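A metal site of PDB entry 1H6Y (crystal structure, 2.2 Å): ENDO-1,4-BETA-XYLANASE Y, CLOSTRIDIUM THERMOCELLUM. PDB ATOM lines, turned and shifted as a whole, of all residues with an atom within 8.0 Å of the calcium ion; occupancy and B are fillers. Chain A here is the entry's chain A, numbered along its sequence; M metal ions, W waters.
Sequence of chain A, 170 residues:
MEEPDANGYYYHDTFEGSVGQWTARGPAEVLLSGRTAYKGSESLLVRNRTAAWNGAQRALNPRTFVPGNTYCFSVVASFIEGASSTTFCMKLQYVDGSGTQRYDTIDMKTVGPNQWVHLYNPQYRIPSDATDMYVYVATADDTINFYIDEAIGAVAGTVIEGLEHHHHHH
The side-chain carboxylate (OE2) of Glu 42 lies within hydrogen-bond range of the backbone NH (N) of Gly 17, 3.2 Å away. The backbone NH of Tyr 38 sits close to the side-chain carboxylate of Asp 149 (2.9 Å). OE1 of Glu 16 lies within hydrogen-bond range of N of Ser 41, at 3.0 Å. The backbone carbonyl oxygen of Val 76 lies within hydrogen-bond range of the backbone NH of Asp 149, at 3.0 Å.
The calcium ion is bound by water W1, the backbone carbonyl oxygen (O) of Thr 14, the side-chain carboxylate (OE2) of Glu 16, the backbone carbonyl oxygen (O) of Lys 39, the backbone carbonyl oxygen (O) of Glu 42, the side-chain carboxylate (OD1) of Asp 149 and the side-chain carboxylate (OD2) of Asp 149.
Within 4 Å of the calcium ion: Thr 14, Glu 16, Lys 39, Glu 42 and Asp 149.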
ATOM      1  N   ASP A  13      32.094 -32.220  17.304  1.00  0.00           N
ATOM      2  CA  ASP A  13      31.355 -31.442  16.330  1.00  0.00           C
ATOM      3  C   ASP A  13      31.033 -30.038  16.803  1.00  0.00           C
ATOM      4  O   ASP A  13      30.233 -29.863  17.733  1.00  0.00           O
ATOM      5  CB  ASP A  13      30.085 -32.181  15.897  1.00  0.00           C
ATOM      6  CG  ASP A  13      30.386 -33.344  14.972  1.00  0.00           C
ATOM      7  OD1 ASP A  13      30.277 -34.514  15.418  1.00  0.00           O
ATOM      8  OD2 ASP A  13      30.790 -33.178  13.798  1.00  0.00           O
ATOM      9  N   THR A  14      31.647 -29.052  16.151  1.00  0.00           N
ATOM     10  CA  THR A  14      31.436 -27.640  16.438  1.00  0.00           C
ATOM     11  C   THR A  14      30.312 -27.118  15.581  1.00  0.00           C
ATOM     12  O   THR A  14      29.779 -26.028  15.828  1.00  0.00           O
ATOM     13  CB  THR A  14      32.683 -26.798  16.053  1.00  0.00           C
ATOM     14  OG1 THR A  14      32.853 -26.878  14.637  1.00  0.00           O
ATOM     15  CG2 THR A  14      33.988 -27.382  16.642  1.00  0.00           C
ATOM     16  N   PHE A  15      29.990 -27.881  14.545  1.00  0.00           N
ATOM     17  CA  PHE A  15      28.996 -27.493  13.544  1.00  0.00           C
ATOM     18  C   PHE A  15      29.315 -26.180  12.801  1.00  0.00           C
ATOM     19  O   PHE A  15      28.452 -25.598  12.136  1.00  0.00           O
ATOM     20  CB  PHE A  15      27.608 -27.563  14.165  1.00  0.00           C
ATOM     21  CG  PHE A  15      27.263 -28.948  14.599  1.00  0.00           C
ATOM     22  CD1 PHE A  15      27.294 -29.319  15.935  1.00  0.00           C
ATOM     23  CD2 PHE A  15      26.995 -29.903  13.657  1.00  0.00           C
ATOM     24  CE1 PHE A  15      27.007 -30.643  16.311  1.00  0.00           C
ATOM     25  CE2 PHE A  15      26.731 -31.180  14.023  1.00  0.00           C
ATOM     26  CZ  PHE A  15      26.716 -31.560  15.347  1.00  0.00           C
ATOM     27  N   GLU A  16      30.578 -25.771  12.860  1.00  0.00           N
ATOM     28  CA  GLU A  16      31.075 -24.587  12.167  1.00  0.00           C
ATOM     29  C   GLU A  16      31.393 -24.964  10.733  1.00  0.00           C
ATOM     30  O   GLU A  16      32.544 -25.137  10.380  1.00  0.00           O
ATOM     31  CB  GLU A  16      32.358 -24.111  12.828  1.00  0.00           C
ATOM     32  CG  GLU A  16      32.162 -23.869  14.299  1.00  0.00           C
ATOM     33  CD  GLU A  16      31.082 -22.847  14.537  1.00  0.00           C
ATOM     34  OE1 GLU A  16      31.065 -21.850  13.788  1.00  0.00           O
ATOM     35  OE2 GLU A  16      30.260 -23.022  15.468  1.00  0.00           O
ATOM     36  N   GLY A  17      30.365 -25.096   9.902  1.00  0.00           N
ATOM     37  CA  GLY A  17      30.562 -25.506   8.516  1.00  0.00           C
ATOM     38  C   GLY A  17      30.315 -26.968   8.126  1.00  0.00           C
ATOM     39  O   GLY A  17      30.341 -27.319   6.937  1.00  0.00           O
ATOM     40  N   SER A  33      22.651 -24.182  11.441  1.00  0.00           N
ATOM     41  CA  SER A  33      21.917 -22.942  11.629  1.00  0.00           C
ATOM     42  C   SER A  33      22.763 -21.893  12.320  1.00  0.00           C
ATOM     43  O   SER A  33      23.520 -22.221  13.240  1.00  0.00           O
ATOM     44  CB  SER A  33      20.651 -23.188  12.457  1.00  0.00           C
ATOM     45  OG  SER A  33      20.052 -21.967  12.855  1.00  0.00           O
ATOM     46  N   THR A  36      21.375 -19.479  16.424  1.00  0.00           N
ATOM     47  CA  THR A  36      21.880 -19.491  17.781  1.00  0.00           C
ATOM     48  C   THR A  36      23.076 -20.452  17.813  1.00  0.00           C
ATOM     49  O   THR A  36      23.219 -21.306  16.934  1.00  0.00           O
ATOM     50  CB  THR A  36      20.760 -19.868  18.784  1.00  0.00           C
ATOM     51  OG1 THR A  36      21.245 -19.801  20.141  1.00  0.00           O
ATOM     52  CG2 THR A  36      20.322 -21.331  18.621  1.00  0.00           C
ATOM     53  N   ALA A  37      23.955 -20.281  18.791  1.00  0.00           N
ATOM     54  CA  ALA A  37      25.121 -21.145  18.859  1.00  0.00           C
ATOM     55  C   ALA A  37      25.698 -21.089  20.235  1.00  0.00           C
ATOM     56  O   ALA A  37      25.549 -20.089  20.936  1.00  0.00           O
ATOM     57  CB  ALA A  37      26.186 -20.726  17.836  1.00  0.00           C
ATOM     58  N   TYR A  38      26.372 -22.153  20.624  1.00  0.00           N
ATOM     59  CA  TYR A  38      26.966 -22.181  21.934  1.00  0.00           C
ATOM     60  C   TYR A  38      28.406 -21.717  21.793  1.00  0.00           C
ATOM     61  O   TYR A  38      28.880 -20.945  22.600  1.00  0.00           O
ATOM     62  CB  TYR A  38      26.855 -23.575  22.536  1.00  0.00           C
ATOM     63  CG  TYR A  38      27.533 -23.709  23.856  1.00  0.00           C
ATOM     64  CD1 TYR A  38      27.021 -23.080  24.984  1.00  0.00           C
ATOM     65  CD2 TYR A  38      28.691 -24.469  23.989  1.00  0.00           C
ATOM     66  CE1 TYR A  38      27.641 -23.207  26.210  1.00  0.00           C
ATOM     67  CE2 TYR A  38      29.321 -24.604  25.195  1.00  0.00           C
ATOM     68  CZ  TYR A  38      28.789 -23.977  26.304  1.00  0.00           C
ATOM     69  OH  TYR A  38      29.420 -24.107  27.518  1.00  0.00           O
ATOM     70  N   LYS A  39      29.104 -22.206  20.779  1.00  0.00           N
ATOM     71  CA  LYS A  39      30.442 -21.747  20.438  1.00  0.00           C
ATOM     72  C   LYS A  39      30.468 -21.536  18.923  1.00  0.00           C
ATOM     73  O   LYS A  39      29.747 -22.217  18.183  1.00  0.00           O
ATOM     74  CB  LYS A  39      31.537 -22.735  20.882  1.00  0.00           C
ATOM     75  CG  LYS A  39      31.837 -22.694  22.362  1.00  0.00           C
ATOM     76  CD  LYS A  39      32.857 -23.783  22.796  1.00  0.00           C
ATOM     77  CE  LYS A  39      33.157 -23.703  24.312  1.00  0.00           C
ATOM     78  NZ  LYS A  39      33.986 -24.854  24.869  1.00  0.00           N
ATOM     79  N   GLY A  40      31.268 -20.583  18.461  1.00  0.00           N
ATOM     80  CA  GLY A  40      31.333 -20.300  17.038  1.00  0.00           C
ATOM     81  C   GLY A  40      30.065 -19.564  16.635  1.00  0.00           C
ATOM     82  O   GLY A  40      29.458 -18.910  17.459  1.00  0.00           O
ATOM     83  N   SER A  41      29.671 -19.667  15.373  1.00  0.00           N
ATOM     84  CA  SER A  41      28.493 -18.942  14.930  1.00  0.00           C
ATOM     85  C   SER A  41      27.381 -19.875  14.496  1.00  0.00           C
ATOM     86  O   SER A  41      26.340 -19.430  14.013  1.00  0.00           O
ATOM     87  CB  SER A  41      28.841 -17.987  13.781  1.00  0.00           C
ATOM     88  OG  SER A  41      29.212 -18.724  12.619  1.00  0.00           O
ATOM     89  N   GLU A  42      27.598 -21.181  14.666  1.00  0.00           N
ATOM     90  CA  GLU A  42      26.592 -22.140  14.260  1.00  0.00           C
ATOM     91  C   GLU A  42      26.317 -23.297  15.220  1.00  0.00           C
ATOM     92  O   GLU A  42      27.112 -23.601  16.108  1.00  0.00           O
ATOM     93  CB  GLU A  42      26.954 -22.717  12.901  1.00  0.00           C
ATOM     94  CG  GLU A  42      26.930 -21.693  11.788  1.00  0.00           C
ATOM     95  CD  GLU A  42      27.014 -22.348  10.442  1.00  0.00           C
ATOM     96  OE1 GLU A  42      25.956 -22.505   9.799  1.00  0.00           O
ATOM     97  OE2 GLU A  42      28.143 -22.741  10.030  1.00  0.00           O
ATOM     98  N   SER A  43      25.178 -23.932  15.015  1.00  0.00           N
ATOM     99  CA  SER A  43      24.816 -25.118  15.753  1.00  0.00           C
ATOM    100  C   SER A  43      24.003 -25.981  14.818  1.00  0.00           C
ATOM    101  O   SER A  43      23.769 -25.608  13.649  1.00  0.00           O
ATOM    102  CB  SER A  43      24.013 -24.782  16.999  1.00  0.00           C
ATOM    103  OG  SER A  43      22.762 -24.224  16.624  1.00  0.00           O
ATOM    104  N   LEU A  44      23.584 -27.134  15.314  1.00  0.00           N
ATOM    105  CA  LEU A  44      22.786 -28.056  14.536  1.00  0.00           C
ATOM    106  C   LEU A  44      21.315 -27.920  14.927  1.00  0.00           C
ATOM    107  O   LEU A  44      20.938 -28.160  16.074  1.00  0.00           O
ATOM    108  CB  LEU A  44      23.266 -29.501  14.751  1.00  0.00           C
ATOM    109  CG  LEU A  44      22.449 -30.473  13.888  1.00  0.00           C
ATOM    110  CD1 LEU A  44      22.897 -30.283  12.442  1.00  0.00           C
ATOM    111  CD2 LEU A  44      22.550 -31.979  14.309  1.00  0.00           C
ATOM    112  N   VAL A  76      25.633 -29.931  24.215  1.00  0.00           N
ATOM    113  CA  VAL A  76      24.864 -28.866  24.830  1.00  0.00           C
ATOM    114  C   VAL A  76      23.662 -28.663  23.938  1.00  0.00           C
ATOM    115  O   VAL A  76      23.747 -28.836  22.723  1.00  0.00           O
ATOM    116  CB  VAL A  76      25.649 -27.547  24.984  1.00  0.00           C
ATOM    117  CG1 VAL A  76      26.869 -27.801  25.836  1.00  0.00           C
ATOM    118  CG2 VAL A  76      26.064 -27.046  23.628  1.00  0.00           C
ATOM    119  N   TRP A 116      21.211 -22.741  27.115  1.00  0.00           N
ATOM    120  CA  TRP A 116      21.978 -23.920  26.754  1.00  0.00           C
ATOM    121  C   TRP A 116      22.095 -24.786  27.992  1.00  0.00           C
ATOM    122  O   TRP A 116      22.302 -24.265  29.090  1.00  0.00           O
ATOM    123  CB  TRP A 116      23.361 -23.532  26.274  1.00  0.00           C
ATOM    124  CG  TRP A 116      23.347 -22.880  24.910  1.00  0.00           C
ATOM    125  CD1 TRP A 116      23.505 -21.536  24.633  1.00  0.00           C
ATOM    126  CD2 TRP A 116      23.183 -23.537  23.655  1.00  0.00           C
ATOM    127  NE1 TRP A 116      23.441 -21.325  23.273  1.00  0.00           N
ATOM    128  CE2 TRP A 116      23.241 -22.539  22.645  1.00  0.00           C
ATOM    129  CE3 TRP A 116      22.971 -24.866  23.270  1.00  0.00           C
ATOM    130  CZ2 TRP A 116      23.111 -22.832  21.282  1.00  0.00           C
ATOM    131  CZ3 TRP A 116      22.837 -25.166  21.913  1.00  0.00           C
ATOM    132  CH2 TRP A 116      22.908 -24.151  20.938  1.00  0.00           C
ATOM    133  N   ILE A 148      21.541 -28.339  18.915  1.00  0.00           N
ATOM    134  CA  ILE A 148      22.631 -28.920  19.683  1.00  0.00           C
ATOM    135  C   ILE A 148      23.967 -28.349  19.175  1.00  0.00           C
ATOM    136  O   ILE A 148      24.085 -27.924  18.012  1.00  0.00           O
ATOM    137  CB  ILE A 148      22.646 -30.461  19.647  1.00  0.00           C
ATOM    138  CG1 ILE A 148      22.991 -30.947  18.231  1.00  0.00           C
ATOM    139  CG2 ILE A 148      21.309 -31.037  20.146  1.00  0.00           C
ATOM    140  CD1 ILE A 148      23.094 -32.452  18.089  1.00  0.00           C
ATOM    141  N   ASP A 149      24.974 -28.385  20.019  1.00  0.00           N
ATOM    142  CA  ASP A 149      26.283 -27.851  19.647  1.00  0.00           C
ATOM    143  C   ASP A 149      27.340 -28.588  20.471  1.00  0.00           C
ATOM    144  O   ASP A 149      27.018 -29.235  21.467  1.00  0.00           O
ATOM    145  CB  ASP A 149      26.323 -26.340  19.947  1.00  0.00           C
ATOM    146  CG  ASP A 149      27.373 -25.580  19.124  1.00  0.00           C
ATOM    147  OD1 ASP A 149      28.108 -26.246  18.363  1.00  0.00           O
ATOM    148  OD2 ASP A 149      27.534 -24.333  19.185  1.00  0.00           O
ATOM    149  N   GLU A 150      28.591 -28.509  20.040  1.00  0.00           N
ATOM    150  CA  GLU A 150      29.695 -29.086  20.804  1.00  0.00           C
ATOM    151  C   GLU A 150      29.432 -30.554  21.185  1.00  0.00           C
ATOM    152  O   GLU A 150      29.518 -30.933  22.364  1.00  0.00           O
ATOM    153  CB  GLU A 150      29.969 -28.254  22.051  1.00  0.00           C
ATOM    154  CG  GLU A 150      30.600 -26.893  21.766  1.00  0.00           C
ATOM    155  CD  GLU A 150      31.920 -27.030  21.011  1.00  0.00           C
ATOM    156  OE1 GLU A 150      31.985 -26.575  19.848  1.00  0.00           O
ATOM    157  OE2 GLU A 150      32.867 -27.606  21.578  1.00  0.00           O
ATOM    158  N   ALA A 151      29.112 -31.373  20.185  1.00  0.00           N
ATOM    159  CA  ALA A 151      28.843 -32.795  20.382  1.00  0.00           C
ATOM    160  C   ALA A 151      30.153 -33.556  20.462  1.00  0.00           C
ATOM    161  O   ALA A 151      30.952 -33.559  19.528  1.00  0.00           O
ATOM    162  CB  ALA A 151      27.980 -33.341  19.249  1.00  0.00           C
HETATM  163 CA    CA M   1      29.129 -24.215  17.131  1.00  0.00          CA
HETATM  164  O   HOH W   1      31.010 -24.573  18.256  1.00  0.00           O
